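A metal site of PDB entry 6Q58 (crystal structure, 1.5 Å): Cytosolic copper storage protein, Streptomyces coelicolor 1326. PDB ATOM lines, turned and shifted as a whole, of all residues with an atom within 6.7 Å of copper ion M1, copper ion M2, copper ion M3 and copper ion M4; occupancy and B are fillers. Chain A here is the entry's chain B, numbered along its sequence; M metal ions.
Residues that only touch copper ion M1: Cys 29. Of the 31 residues printed, 4 come within 4 Å of copper ion M1. The nearest printed residue that does not touch copper ion M1 is Cys 41 (4.7 Å).
SG of Cys 98 binds copper ion M2, 2.1 Å away. The side-chain sulfur (SG) of Cys 41 is bound to copper ion M2. Copper ion M2 has two donor atoms within binding distance.
Copper ion M3 is bound by SG of Cys 88 (2.0 Å) and SG of Cys 25 (2.2 Å). Copper ion M3 has two donor atoms within binding distance.
N of Ala 26 is in hydrogen-bond range of OD2 of Asp 45, 3.1 Å away. SG of Cys 29 is in hydrogen-bond range of O of Cys 25, 3.4 Å away. O of Thr 44 is in hydrogen-bond range of SG of Cys 84. The side-chain sulfur of Cys 101 is in hydrogen-bond range of the backbone carbonyl oxygen of Ala 21 (3.8 Å). SG of Cys 88 sits close to OD1 of Asp 45 (3.6 Å). The backbone carbonyl oxygen of Cys 101 lies within hydrogen-bond range of the side-chain sulfur of Cys 105. The side-chain sulfur of Cys 88 sits close to the side-chain sulfur of Cys 101 (3.7 Å). OD2 of Asp 45 sits close to SG of Cys 41 (3.6 Å).
Asp 45 touches copper ion M4. Cys 84 touches copper ion M4 (O to CU, 3.999 Å). The nearest printed residue that does not touch copper ion M4 is Glu 87 (4.04 Å).
Copper ion M1 is bound by a ring nitrogen (ND1) of His 97, the side-chain sulfur (SG) of Cys 25 and the side-chain sulfur (SG) of Cys 98. Copper ion M1 has three donor atoms within binding distance.
SG of Cys 29 touches copper ion M2 (3.6 Å). Within 4 Å of copper ion M2: Cys 25, Cys 29, Cys 41, Cys 88 and Cys 98.
OD1 of Asp 45 touches copper ion M3 (3.2 Å). Cys 101 touches copper ion M3. The nearest printed residue that does not touch copper ion M3 is His 97 (4.5 Å).
Copper ion M4 is bound by the side-chain sulfur of Cys 41 (2.1 Å) and the side-chain sulfur of Cys 88 (2.1 Å). Copper ion M4 has two donor atoms within binding distance.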
ATOM      1  N   ALA A  21      -5.844 -12.152  25.298  1.00  0.00           N
ATOM      2  CA  ALA A  21      -5.371 -13.537  25.144  1.00  0.00           C
ATOM      3  C   ALA A  21      -5.875 -14.397  26.307  1.00  0.00           C
ATOM      4  O   ALA A  21      -6.336 -15.507  26.096  1.00  0.00           O
ATOM      5  CB  ALA A  21      -3.850 -13.594  25.047  1.00  0.00           C
ATOM      6  N   CYS A  22      -5.802 -13.837  27.515  1.00  0.00           N
ATOM      7  CA  CYS A  22      -6.272 -14.549  28.702  1.00  0.00           C
ATOM      8  C   CYS A  22      -7.769 -14.780  28.675  1.00  0.00           C
ATOM      9  O   CYS A  22      -8.265 -15.829  29.060  1.00  0.00           O
ATOM     10  CB  CYS A  22      -5.867 -13.811  29.963  1.00  0.00           C
ATOM     11  SG  CYS A  22      -4.123 -13.879  30.332  1.00  0.00           S
ATOM     12  N   ALA A  24      -9.618 -15.006  25.972  1.00  0.00           N
ATOM     13  CA  ALA A  24      -9.844 -16.014  24.948  1.00  0.00           C
ATOM     14  C   ALA A  24      -9.552 -17.419  25.457  1.00  0.00           C
ATOM     15  O   ALA A  24     -10.292 -18.347  25.211  1.00  0.00           O
ATOM     16  CB  ALA A  24      -9.025 -15.702  23.706  1.00  0.00           C
ATOM     17  N   CYS A  25      -8.460 -17.547  26.206  1.00  0.00           N
ATOM     18  CA  CYS A  25      -8.105 -18.853  26.773  1.00  0.00           C
ATOM     19  C   CYS A  25      -9.120 -19.300  27.801  1.00  0.00           C
ATOM     20  O   CYS A  25      -9.561 -20.471  27.794  1.00  0.00           O
ATOM     21  CB  CYS A  25      -6.720 -18.764  27.356  1.00  0.00           C
ATOM     22  SG  CYS A  25      -6.181 -20.294  28.228  1.00  0.00           S
ATOM     23  N   ALA A  26      -9.537 -18.403  28.690  1.00  0.00           N
ATOM     24  CA  ALA A  26     -10.525 -18.781  29.696  1.00  0.00           C
ATOM     25  C   ALA A  26     -11.805 -19.330  29.018  1.00  0.00           C
ATOM     26  O   ALA A  26     -12.361 -20.328  29.418  1.00  0.00           O
ATOM     27  CB  ALA A  26     -10.843 -17.617  30.597  1.00  0.00           C
ATOM     28  N   ALA A  28     -12.130 -20.599  25.961  1.00  0.00           N
ATOM     29  CA  ALA A  28     -11.827 -21.879  25.312  1.00  0.00           C
ATOM     30  C   ALA A  28     -11.818 -23.001  26.362  1.00  0.00           C
ATOM     31  O   ALA A  28     -12.351 -24.077  26.128  1.00  0.00           O
ATOM     32  CB  ALA A  28     -10.504 -21.848  24.567  1.00  0.00           C
ATOM     33  N   CYS A  29     -11.223 -22.739  27.513  1.00  0.00           N
ATOM     34  CA  CYS A  29     -11.214 -23.749  28.593  1.00  0.00           C
ATOM     35  C   CYS A  29     -12.638 -24.093  29.059  1.00  0.00           C
ATOM     36  O   CYS A  29     -12.966 -25.246  29.333  1.00  0.00           O
ATOM     37  CB  CYS A  29     -10.400 -23.263  29.787  1.00  0.00           C
ATOM     38  SG  CYS A  29      -8.649 -23.285  29.559  1.00  0.00           S
ATOM     39  N   LEU A  38      -9.449 -27.591  34.316  1.00  0.00           N
ATOM     40  CA  LEU A  38      -8.897 -26.334  33.830  1.00  0.00           C
ATOM     41  C   LEU A  38      -9.344 -25.144  34.676  1.00  0.00           C
ATOM     42  O   LEU A  38      -9.209 -23.994  34.258  1.00  0.00           O
ATOM     43  CB  LEU A  38      -9.353 -26.131  32.384  1.00  0.00           C
ATOM     44  CG  LEU A  38      -8.825 -27.180  31.387  1.00  0.00           C
ATOM     45  CD1 LEU A  38      -9.517 -27.034  30.062  1.00  0.00           C
ATOM     46  CD2 LEU A  38      -7.305 -27.041  31.228  1.00  0.00           C
ATOM     47  N   LYS A  40      -8.269 -23.807  37.570  1.00  0.00           N
ATOM     48  CA  LYS A  40      -7.197 -22.872  37.990  1.00  0.00           C
ATOM     49  C   LYS A  40      -6.705 -22.054  36.805  1.00  0.00           C
ATOM     50  O   LYS A  40      -6.468 -20.827  36.979  1.00  0.00           O
ATOM     51  CB  LYS A  40      -6.030 -23.597  38.679  1.00  0.00           C
ATOM     52  CG  LYS A  40      -4.934 -22.664  39.167  1.00  0.00           C
ATOM     53  CD  LYS A  40      -3.901 -23.306  40.065  1.00  0.00           C
ATOM     54  CE  LYS A  40      -2.949 -22.249  40.618  1.00  0.00           C
ATOM     55  NZ  LYS A  40      -1.917 -22.962  41.405  1.00  0.00           N
ATOM     56  N   CYS A  41      -6.611 -22.647  35.629  1.00  0.00           N
ATOM     57  CA  CYS A  41      -6.264 -21.908  34.437  1.00  0.00           C
ATOM     58  C   CYS A  41      -7.272 -20.748  34.202  1.00  0.00           C
ATOM     59  O   CYS A  41      -6.881 -19.584  34.012  1.00  0.00           O
ATOM     60  CB  CYS A  41      -6.223 -22.844  33.245  1.00  0.00           C
ATOM     61  SG  CYS A  41      -5.723 -21.949  31.794  1.00  0.00           S
ATOM     62  N   ILE A  42      -8.543 -21.089  34.207  1.00  0.00           N
ATOM     63  CA  ILE A  42      -9.595 -20.108  34.018  1.00  0.00           C
ATOM     64  C   ILE A  42      -9.498 -18.984  35.057  1.00  0.00           C
ATOM     65  O   ILE A  42      -9.533 -17.805  34.711  1.00  0.00           O
ATOM     66  CB  ILE A  42     -10.984 -20.746  34.016  1.00  0.00           C
ATOM     67  CG1 ILE A  42     -11.135 -21.657  32.804  1.00  0.00           C
ATOM     68  CG2 ILE A  42     -12.066 -19.675  33.993  1.00  0.00           C
ATOM     69  CD1 ILE A  42     -12.240 -22.713  32.950  1.00  0.00           C
ATOM     70  N   THR A  44      -6.964 -18.017  36.909  1.00  0.00           N
ATOM     71  CA  THR A  44      -5.744 -17.226  36.780  1.00  0.00           C
ATOM     72  C   THR A  44      -5.796 -16.349  35.519  1.00  0.00           C
ATOM     73  O   THR A  44      -5.299 -15.210  35.530  1.00  0.00           O
ATOM     74  CB  THR A  44      -4.482 -18.107  36.870  1.00  0.00           C
ATOM     75  OG1 THR A  44      -4.613 -18.995  37.999  1.00  0.00           O
ATOM     76  CG2 THR A  44      -3.283 -17.291  37.024  1.00  0.00           C
ATOM     77  N   ASP A  45      -6.408 -16.864  34.452  1.00  0.00           N
ATOM     78  CA  ASP A  45      -6.678 -16.061  33.252  1.00  0.00           C
ATOM     79  C   ASP A  45      -7.485 -14.816  33.626  1.00  0.00           C
ATOM     80  O   ASP A  45      -7.200 -13.733  33.117  1.00  0.00           O
ATOM     81  CB  ASP A  45      -7.503 -16.825  32.209  1.00  0.00           C
ATOM     82  CG  ASP A  45      -6.726 -17.962  31.510  1.00  0.00           C
ATOM     83  OD1 ASP A  45      -5.509 -17.952  31.426  1.00  0.00           O
ATOM     84  OD2 ASP A  45      -7.430 -18.855  30.945  1.00  0.00           O
ATOM     85  N   ALA A  83       2.411 -16.110  36.864  1.00  0.00           N
ATOM     86  CA  ALA A  83       1.539 -17.161  37.403  1.00  0.00           C
ATOM     87  C   ALA A  83       0.609 -17.693  36.327  1.00  0.00           C
ATOM     88  O   ALA A  83       0.390 -18.920  36.238  1.00  0.00           O
ATOM     89  CB  ALA A  83       0.752 -16.659  38.585  1.00  0.00           C
ATOM     90  N   CYS A  84       0.022 -16.809  35.538  1.00  0.00           N
ATOM     91  CA  CYS A  84      -0.903 -17.252  34.516  1.00  0.00           C
ATOM     92  C   CYS A  84      -0.165 -18.056  33.459  1.00  0.00           C
ATOM     93  O   CYS A  84      -0.617 -19.099  33.001  1.00  0.00           O
ATOM     94  CB  CYS A  84      -1.638 -16.041  33.923  1.00  0.00           C
ATOM     95  SG  CYS A  84      -3.021 -16.515  32.883  1.00  0.00           S
ATOM     96  N   GLY A  85       1.008 -17.572  33.047  1.00  0.00           N
ATOM     97  CA  GLY A  85       1.832 -18.286  32.093  1.00  0.00           C
ATOM     98  C   GLY A  85       2.212 -19.649  32.592  1.00  0.00           C
ATOM     99  O   GLY A  85       2.177 -20.589  31.829  1.00  0.00           O
ATOM    100  N   ASP A  86       2.564 -19.758  33.851  1.00  0.00           N
ATOM    101  CA  ASP A  86       2.893 -21.072  34.430  1.00  0.00           C
ATOM    102  C   ASP A  86       1.730 -22.037  34.312  1.00  0.00           C
ATOM    103  O   ASP A  86       1.923 -23.186  33.951  1.00  0.00           O
ATOM    104  CB  ASP A  86       3.298 -20.961  35.909  1.00  0.00           C
ATOM    105  CG  ASP A  86       4.618 -20.253  36.146  1.00  0.00           C
ATOM    106  OD1 ASP A  86       5.318 -19.906  35.174  1.00  0.00           O
ATOM    107  OD2 ASP A  86       4.887 -19.995  37.316  1.00  0.00           O
ATOM    108  N   GLU A  87       0.523 -21.581  34.624  1.00  0.00           N
ATOM    109  CA  GLU A  87      -0.647 -22.506  34.655  1.00  0.00           C
ATOM    110  C   GLU A  87      -1.021 -22.848  33.211  1.00  0.00           C
ATOM    111  O   GLU A  87      -1.253 -24.028  32.891  1.00  0.00           O
ATOM    112  CB  GLU A  87      -1.790 -21.894  35.413  1.00  0.00           C
ATOM    113  CG  GLU A  87      -2.997 -22.791  35.570  1.00  0.00           C
ATOM    114  CD  GLU A  87      -2.770 -24.071  36.362  1.00  0.00           C
ATOM    115  OE1 GLU A  87      -1.803 -24.207  37.129  1.00  0.00           O
ATOM    116  OE2 GLU A  87      -3.595 -24.982  36.270  1.00  0.00           O
ATOM    117  N   CYS A  88      -1.016 -21.892  32.308  1.00  0.00           N
ATOM    118  CA  CYS A  88      -1.253 -22.193  30.887  1.00  0.00           C
ATOM    119  C   CYS A  88      -0.212 -23.142  30.317  1.00  0.00           C
ATOM    120  O   CYS A  88      -0.538 -24.060  29.585  1.00  0.00           O
ATOM    121  CB  CYS A  88      -1.252 -20.943  30.046  1.00  0.00           C
ATOM    122  SG  CYS A  88      -2.665 -19.795  30.362  1.00  0.00           S
ATOM    123  N   ALA A  89       1.025 -22.954  30.687  1.00  0.00           N
ATOM    124  CA  ALA A  89       2.127 -23.818  30.158  1.00  0.00           C
ATOM    125  C   ALA A  89       1.919 -25.281  30.586  1.00  0.00           C
ATOM    126  O   ALA A  89       2.296 -26.168  29.848  1.00  0.00           O
ATOM    127  CB  ALA A  89       3.460 -23.305  30.633  1.00  0.00           C
ATOM    128  N   HIS A  91      -0.813 -26.850  30.571  1.00  0.00           N
ATOM    129  CA  HIS A  91      -1.830 -27.382  29.677  1.00  0.00           C
ATOM    130  C   HIS A  91      -1.520 -27.226  28.195  1.00  0.00           C
ATOM    131  O   HIS A  91      -2.307 -27.648  27.377  1.00  0.00           O
ATOM    132  CB  HIS A  91      -3.171 -26.719  29.994  1.00  0.00           C
ATOM    133  CG  HIS A  91      -3.643 -27.031  31.360  1.00  0.00           C
ATOM    134  ND1 HIS A  91      -3.812 -26.071  32.327  1.00  0.00           N
ATOM    135  CD2 HIS A  91      -3.970 -28.210  31.932  1.00  0.00           C
ATOM    136  CE1 HIS A  91      -4.219 -26.658  33.445  1.00  0.00           C
ATOM    137  NE2 HIS A  91      -4.357 -27.954  33.220  1.00  0.00           N
ATOM    138  N   ALA A  92      -0.371 -26.627  27.886  1.00  0.00           N
ATOM    139  CA  ALA A  92      -0.050 -26.225  26.527  1.00  0.00           C
ATOM    140  C   ALA A  92       0.152 -27.410  25.588  1.00  0.00           C
ATOM    141  O   ALA A  92      -0.092 -27.285  24.390  1.00  0.00           O
ATOM    142  CB  ALA A  92       1.160 -25.320  26.505  1.00  0.00           C
ATOM    143  N   HIS A  95      -3.587 -28.332  24.877  1.00  0.00           N
ATOM    144  CA  HIS A  95      -4.452 -27.284  24.374  1.00  0.00           C
ATOM    145  C   HIS A  95      -3.694 -26.131  23.748  1.00  0.00           C
ATOM    146  O   HIS A  95      -2.995 -25.414  24.424  1.00  0.00           O
ATOM    147  CB  HIS A  95      -5.334 -26.721  25.493  1.00  0.00           C
ATOM    148  CG  HIS A  95      -6.198 -27.740  26.133  1.00  0.00           C
ATOM    149  ND1 HIS A  95      -6.122 -28.065  27.460  1.00  0.00           N
ATOM    150  CD2 HIS A  95      -7.159 -28.531  25.609  1.00  0.00           C
ATOM    151  CE1 HIS A  95      -6.997 -29.030  27.722  1.00  0.00           C
ATOM    152  NE2 HIS A  95      -7.644 -29.318  26.613  1.00  0.00           N
ATOM    153  N   GLU A  96      -3.864 -25.957  22.447  1.00  0.00           N
ATOM    154  CA  GLU A  96      -3.225 -24.862  21.739  1.00  0.00           C
ATOM    155  C   GLU A  96      -3.598 -23.492  22.304  1.00  0.00           C
ATOM    156  O   GLU A  96      -2.758 -22.599  22.366  1.00  0.00           O
ATOM    157  CB  GLU A  96      -3.568 -24.945  20.239  1.00  0.00           C
ATOM    158  CG  GLU A  96      -2.841 -23.955  19.342  1.00  0.00           C
ATOM    159  CD  GLU A  96      -1.334 -24.176  19.273  1.00  0.00           C
ATOM    160  OE1 GLU A  96      -0.816 -25.252  19.712  1.00  0.00           O
ATOM    161  OE2 GLU A  96      -0.669 -23.241  18.769  1.00  0.00           O
ATOM    162  N   HIS A  97      -4.841 -23.322  22.748  1.00  0.00           N
ATOM    163  CA  HIS A  97      -5.252 -22.066  23.356  1.00  0.00           C
ATOM    164  C   HIS A  97      -4.401 -21.713  24.589  1.00  0.00           C
ATOM    165  O   HIS A  97      -4.086 -20.559  24.804  1.00  0.00           O
ATOM    166  CB  HIS A  97      -6.774 -21.975  23.630  1.00  0.00           C
ATOM    167  CG  HIS A  97      -7.368 -23.147  24.365  1.00  0.00           C
ATOM    168  ND1 HIS A  97      -7.351 -23.268  25.738  1.00  0.00           N
ATOM    169  CD2 HIS A  97      -8.082 -24.203  23.909  1.00  0.00           C
ATOM    170  CE1 HIS A  97      -8.005 -24.351  26.098  1.00  0.00           C
ATOM    171  NE2 HIS A  97      -8.460 -24.941  25.011  1.00  0.00           N
ATOM    172  N   CYS A  98      -4.040 -22.722  25.379  1.00  0.00           N
ATOM    173  CA  CYS A  98      -3.184 -22.507  26.538  1.00  0.00           C
ATOM    174  C   CYS A  98      -1.746 -22.208  26.089  1.00  0.00           C
ATOM    175  O   CYS A  98      -1.066 -21.396  26.708  1.00  0.00           O
ATOM    176  CB  CYS A  98      -3.252 -23.707  27.484  1.00  0.00           C
ATOM    177  SG  CYS A  98      -4.912 -23.950  28.229  1.00  0.00           S
ATOM    178  N   ARG A  99      -1.266 -22.846  25.019  1.00  0.00           N
ATOM    179  CA  ARG A  99       0.085 -22.525  24.498  1.00  0.00           C
ATOM    180  C   ARG A  99       0.140 -21.074  24.056  1.00  0.00           C
ATOM    181  O   ARG A  99       1.085 -20.364  24.375  1.00  0.00           O
ATOM    182  CB  ARG A  99       0.412 -23.456  23.318  1.00  0.00           C
ATOM    183  CG  ARG A  99       1.850 -23.313  22.852  1.00  0.00           C
ATOM    184  CD  ARG A  99       2.076 -23.961  21.480  1.00  0.00           C
ATOM    185  NE  ARG A  99       1.492 -23.177  20.396  1.00  0.00           N
ATOM    186  CZ  ARG A  99       1.943 -21.990  19.977  1.00  0.00           C
ATOM    187  NH1 ARG A  99       3.038 -21.423  20.492  1.00  0.00           N
ATOM    188  NH2 ARG A  99       1.306 -21.374  18.995  1.00  0.00           N
ATOM    189  N   VAL A 100      -0.868 -20.633  23.332  1.00  0.00           N
ATOM    190  CA  VAL A 100      -0.922 -19.266  22.816  1.00  0.00           C
ATOM    191  C   VAL A 100      -0.985 -18.270  23.973  1.00  0.00           C
ATOM    192  O   VAL A 100      -0.278 -17.264  24.014  1.00  0.00           O
ATOM    193  CB  VAL A 100      -2.115 -19.098  21.853  1.00  0.00           C
ATOM    194  CG1 VAL A 100      -2.380 -17.644  21.534  1.00  0.00           C
ATOM    195  CG2 VAL A 100      -1.889 -19.892  20.584  1.00  0.00           C
ATOM    196  N   CYS A 101      -1.823 -18.562  24.950  1.00  0.00           N
ATOM    197  CA  CYS A 101      -1.952 -17.709  26.093  1.00  0.00           C
ATOM    198  C   CYS A 101      -0.669 -17.629  26.902  1.00  0.00           C
ATOM    199  O   CYS A 101      -0.250 -16.562  27.328  1.00  0.00           O
ATOM    200  CB  CYS A 101      -3.105 -18.153  26.944  1.00  0.00           C
ATOM    201  SG  CYS A 101      -3.499 -16.902  28.204  1.00  0.00           S
ATOM    202  N   ALA A 102      -0.004 -18.753  27.101  1.00  0.00           N
ATOM    203  CA  ALA A 102       1.292 -18.755  27.824  1.00  0.00           C
ATOM    204  C   ALA A 102       2.278 -17.831  27.175  1.00  0.00           C
ATOM    205  O   ALA A 102       2.964 -17.089  27.874  1.00  0.00           O
ATOM    206  CB  ALA A 102       1.872 -20.161  27.938  1.00  0.00           C
ATOM    207  N   CYS A 105       1.369 -14.255  27.944  1.00  0.00           N
ATOM    208  CA  CYS A 105       1.683 -13.937  29.337  1.00  0.00           C
ATOM    209  C   CYS A 105       3.171 -13.735  29.529  1.00  0.00           C
ATOM    210  O   CYS A 105       3.590 -12.821  30.248  1.00  0.00           O
ATOM    211  CB  CYS A 105       1.205 -15.038  30.290  1.00  0.00           C
ATOM    212  SG  CYS A 105      -0.607 -15.118  30.473  1.00  0.00           S
HETATM  213 CU    CU M   1      -6.344 -22.309  27.196  1.00  0.00          CU
HETATM  214 CU    CU M   2      -5.106 -22.932  30.039  1.00  0.00          CU
HETATM  215 CU    CU M   3      -4.322 -20.064  29.298  1.00  0.00          CU
HETATM  216 CU    CU M   4      -4.066 -20.654  31.704  1.00  0.00          CU
